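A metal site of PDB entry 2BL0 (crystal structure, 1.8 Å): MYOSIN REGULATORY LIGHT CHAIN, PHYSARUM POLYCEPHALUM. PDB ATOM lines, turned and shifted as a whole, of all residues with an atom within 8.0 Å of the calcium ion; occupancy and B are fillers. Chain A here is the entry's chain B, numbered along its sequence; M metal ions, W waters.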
ATOM      1  N   PHE A  11      23.894  20.100   0.650  1.00  0.00           N
ATOM      2  CA  PHE A  11      23.487  21.309  -0.040  1.00  0.00           C
ATOM      3  C   PHE A  11      23.692  22.538   0.838  1.00  0.00           C
ATOM      4  O   PHE A  11      24.241  23.542   0.391  1.00  0.00           O
ATOM      5  CB  PHE A  11      22.034  21.216  -0.497  1.00  0.00           C
ATOM      6  CG  PHE A  11      21.572  22.416  -1.291  1.00  0.00           C
ATOM      7  CD1 PHE A  11      21.693  22.430  -2.694  1.00  0.00           C
ATOM      8  CD2 PHE A  11      21.008  23.498  -0.661  1.00  0.00           C
ATOM      9  CE1 PHE A  11      21.293  23.525  -3.426  1.00  0.00           C
ATOM     10  CE2 PHE A  11      20.595  24.582  -1.388  1.00  0.00           C
ATOM     11  CZ  PHE A  11      20.729  24.606  -2.761  1.00  0.00           C
ATOM     12  N   GLN A  12      23.278  22.443   2.093  1.00  0.00           N
ATOM     13  CA  GLN A  12      23.375  23.553   3.021  1.00  0.00           C
ATOM     14  C   GLN A  12      24.839  23.953   3.262  1.00  0.00           C
ATOM     15  O   GLN A  12      25.139  25.121   3.446  1.00  0.00           O
ATOM     16  CB  GLN A  12      22.692  23.231   4.354  1.00  0.00           C
ATOM     17  CG  GLN A  12      21.203  23.086   4.202  1.00  0.00           C
ATOM     18  CD  GLN A  12      20.489  22.776   5.488  1.00  0.00           C
ATOM     19  OE1 GLN A  12      19.320  23.121   5.621  1.00  0.00           O
ATOM     20  NE2 GLN A  12      21.167  22.127   6.435  1.00  0.00           N
ATOM     21  N   PHE A  14      27.275  23.709   1.017  1.00  0.00           N
ATOM     22  CA  PHE A  14      27.657  24.423  -0.191  1.00  0.00           C
ATOM     23  C   PHE A  14      26.994  25.798  -0.279  1.00  0.00           C
ATOM     24  O   PHE A  14      27.566  26.713  -0.860  1.00  0.00           O
ATOM     25  CB  PHE A  14      27.328  23.612  -1.444  1.00  0.00           C
ATOM     26  CG  PHE A  14      28.386  22.612  -1.800  1.00  0.00           C
ATOM     27  CD1 PHE A  14      28.467  21.378  -1.169  1.00  0.00           C
ATOM     28  CD2 PHE A  14      29.323  22.912  -2.786  1.00  0.00           C
ATOM     29  CE1 PHE A  14      29.474  20.464  -1.495  1.00  0.00           C
ATOM     30  CE2 PHE A  14      30.317  22.025  -3.105  1.00  0.00           C
ATOM     31  CZ  PHE A  14      30.404  20.796  -2.469  1.00  0.00           C
ATOM     32  N   ASP A  15      25.801  25.942   0.296  1.00  0.00           N
ATOM     33  CA  ASP A  15      25.038  27.196   0.234  1.00  0.00           C
ATOM     34  C   ASP A  15      25.492  28.067   1.402  1.00  0.00           C
ATOM     35  O   ASP A  15      24.781  28.234   2.400  1.00  0.00           O
ATOM     36  CB  ASP A  15      23.546  26.898   0.305  1.00  0.00           C
ATOM     37  CG  ASP A  15      22.678  28.137   0.214  1.00  0.00           C
ATOM     38  OD1 ASP A  15      23.136  29.168  -0.330  1.00  0.00           O
ATOM     39  OD2 ASP A  15      21.490  28.139   0.620  1.00  0.00           O
ATOM     40  N   LYS A  16      26.685  28.632   1.258  1.00  0.00           N
ATOM     41  CA  LYS A  16      27.327  29.338   2.373  1.00  0.00           C
ATOM     42  C   LYS A  16      26.542  30.577   2.825  1.00  0.00           C
ATOM     43  O   LYS A  16      26.527  30.904   4.018  1.00  0.00           O
ATOM     44  CB  LYS A  16      28.753  29.694   1.978  1.00  0.00           C
ATOM     45  CG  LYS A  16      29.686  28.456   1.966  1.00  0.00           C
ATOM     46  CD  LYS A  16      31.167  28.855   1.919  1.00  0.00           C
ATOM     47  CE  LYS A  16      32.070  27.678   1.508  1.00  0.00           C
ATOM     48  NZ  LYS A  16      32.775  27.916   0.209  1.00  0.00           N
ATOM     49  N   ASP A  17      25.861  31.243   1.884  1.00  0.00           N
ATOM     50  CA  ASP A  17      25.093  32.470   2.192  1.00  0.00           C
ATOM     51  C   ASP A  17      23.600  32.215   2.466  1.00  0.00           C
ATOM     52  O   ASP A  17      22.835  33.149   2.706  1.00  0.00           O
ATOM     53  CB  ASP A  17      25.322  33.553   1.110  1.00  0.00           C
ATOM     54  CG  ASP A  17      24.679  33.218  -0.214  1.00  0.00           C
ATOM     55  OD1 ASP A  17      24.306  32.063  -0.432  1.00  0.00           O
ATOM     56  OD2 ASP A  17      24.505  34.061  -1.133  1.00  0.00           O
ATOM     57  N   ASN A  18      23.195  30.948   2.465  1.00  0.00           N
ATOM     58  CA  ASN A  18      21.872  30.539   2.951  1.00  0.00           C
ATOM     59  C   ASN A  18      20.694  31.125   2.163  1.00  0.00           C
ATOM     60  O   ASN A  18      19.641  31.407   2.723  1.00  0.00           O
ATOM     61  CB  ASN A  18      21.702  30.871   4.439  1.00  0.00           C
ATOM     62  CG  ASN A  18      22.778  30.253   5.295  1.00  0.00           C
ATOM     63  OD1 ASN A  18      23.547  30.951   5.942  1.00  0.00           O
ATOM     64  ND2 ASN A  18      22.827  28.934   5.318  1.00  0.00           N
ATOM     65  N   ASP A  19      20.878  31.303   0.856  1.00  0.00           N
ATOM     66  CA  ASP A  19      19.794  31.849   0.021  1.00  0.00           C
ATOM     67  C   ASP A  19      19.031  30.760  -0.746  1.00  0.00           C
ATOM     68  O   ASP A  19      18.141  31.062  -1.519  1.00  0.00           O
ATOM     69  CB  ASP A  19      20.294  32.975  -0.891  1.00  0.00           C
ATOM     70  CG  ASP A  19      21.106  32.496  -2.061  1.00  0.00           C
ATOM     71  OD1 ASP A  19      21.591  31.352  -2.092  1.00  0.00           O
ATOM     72  OD2 ASP A  19      21.319  33.223  -3.050  1.00  0.00           O
ATOM     73  N   GLY A  20      19.365  29.493  -0.508  1.00  0.00           N
ATOM     74  CA  GLY A  20      18.705  28.388  -1.166  1.00  0.00           C
ATOM     75  C   GLY A  20      19.212  28.052  -2.548  1.00  0.00           C
ATOM     76  O   GLY A  20      18.623  27.192  -3.226  1.00  0.00           O
ATOM     77  N   LYS A  21      20.306  28.693  -2.963  1.00  0.00           N
ATOM     78  CA  LYS A  21      20.898  28.484  -4.291  1.00  0.00           C
ATOM     79  C   LYS A  21      22.381  28.181  -4.215  1.00  0.00           C
ATOM     80  O   LYS A  21      23.101  28.744  -3.396  1.00  0.00           O
ATOM     81  CB  LYS A  21      20.685  29.701  -5.177  1.00  0.00           C
ATOM     82  CG  LYS A  21      19.233  30.034  -5.467  1.00  0.00           C
ATOM     83  CD  LYS A  21      18.541  28.995  -6.320  1.00  0.00           C
ATOM     84  CE  LYS A  21      17.873  29.600  -7.545  1.00  0.00           C
ATOM     85  NZ  LYS A  21      17.245  30.890  -7.270  1.00  0.00           N
ATOM     86  N   VAL A  22      22.845  27.304  -5.091  1.00  0.00           N
ATOM     87  CA  VAL A  22      24.263  26.975  -5.176  1.00  0.00           C
ATOM     88  C   VAL A  22      24.658  27.147  -6.633  1.00  0.00           C
ATOM     89  O   VAL A  22      23.892  26.797  -7.524  1.00  0.00           O
ATOM     90  CB  VAL A  22      24.547  25.534  -4.663  1.00  0.00           C
ATOM     91  CG1 VAL A  22      25.919  25.105  -5.004  1.00  0.00           C
ATOM     92  CG2 VAL A  22      24.313  25.461  -3.140  1.00  0.00           C
ATOM     93  N   SER A  23      25.833  27.734  -6.881  1.00  0.00           N
ATOM     94  CA  SER A  23      26.320  27.984  -8.233  1.00  0.00           C
ATOM     95  C   SER A  23      26.385  26.686  -8.994  1.00  0.00           C
ATOM     96  O   SER A  23      26.759  25.663  -8.435  1.00  0.00           O
ATOM     97  CB  SER A  23      27.721  28.583  -8.202  1.00  0.00           C
ATOM     98  OG  SER A  23      28.277  28.612  -9.516  1.00  0.00           O
ATOM     99  N   GLU A  54      22.609  28.640 -11.443  1.00  0.00           N
ATOM    100  CA  GLU A  54      22.534  28.091 -10.076  1.00  0.00           C
ATOM    101  C   GLU A  54      21.460  27.026  -9.973  1.00  0.00           C
ATOM    102  O   GLU A  54      20.628  26.888 -10.879  1.00  0.00           O
ATOM    103  CB  GLU A  54      22.271  29.200  -9.040  1.00  0.00           C
ATOM    104  CG  GLU A  54      21.777  30.492  -9.626  1.00  0.00           C
ATOM    105  CD  GLU A  54      21.292  31.479  -8.587  1.00  0.00           C
ATOM    106  OE1 GLU A  54      20.227  32.100  -8.825  1.00  0.00           O
ATOM    107  OE2 GLU A  54      21.981  31.652  -7.560  1.00  0.00           O
ATOM    108  N   PHE A  55      21.489  26.262  -8.886  1.00  0.00           N
ATOM    109  CA  PHE A  55      20.480  25.232  -8.643  1.00  0.00           C
ATOM    110  C   PHE A  55      20.027  25.224  -7.184  1.00  0.00           C
ATOM    111  O   PHE A  55      20.777  25.617  -6.299  1.00  0.00           O
ATOM    112  CB  PHE A  55      20.984  23.839  -9.052  1.00  0.00           C
ATOM    113  CG  PHE A  55      22.206  23.364  -8.292  1.00  0.00           C
ATOM    114  CD1 PHE A  55      23.484  23.743  -8.686  1.00  0.00           C
ATOM    115  CD2 PHE A  55      22.062  22.528  -7.195  1.00  0.00           C
ATOM    116  CE1 PHE A  55      24.613  23.273  -7.966  1.00  0.00           C
ATOM    117  CE2 PHE A  55      23.183  22.061  -6.486  1.00  0.00           C
ATOM    118  CZ  PHE A  55      24.451  22.459  -6.869  1.00  0.00           C
HETATM  119 CA    CA M   1      23.820  30.419  -2.044  1.00  0.00          CA
HETATM  120  O   HOH W   1      24.176  31.737  -3.792  1.00  0.00           O
HETATM  121  O   HOH W   2      25.928  29.612  -2.404  1.00  0.00           O
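N of Asn 18 lies close to OD1 of Asp 15, at 3.3 Å.
NZ of Lys 21 lies within salt-bridge range of OE1 of Glu 54 (3.6 Å).
The side-chain carboxylate (OD2) of Asp 15 lies within hydrogen-bond range of the backbone NH (N) of Gly 20, 2.8 Å away.
Of the 14 residues printed, 4 come within 4 Å of the calcium ion.
The nearest printed residue that does not touch the calcium ion is Val 22 (4.5 Å).
The calcium ion is bound by water W1 (2.2 Å).
The calcium ion is bound by the side-chain carboxylate (OD1) of Asp 15 (2.2 Å).
O of Lys 21 is bound to the calcium ion, at 2.3 Å.
Water W2 binds the calcium ion (2.3 Å).
The side-chain carboxylate (OD1) of Asp 17 binds the calcium ion (2.4 Å).
The calcium ion is bound by OD1 of Asp 19 (2.4 Å).
The calcium ion has six donor atoms within binding distance.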
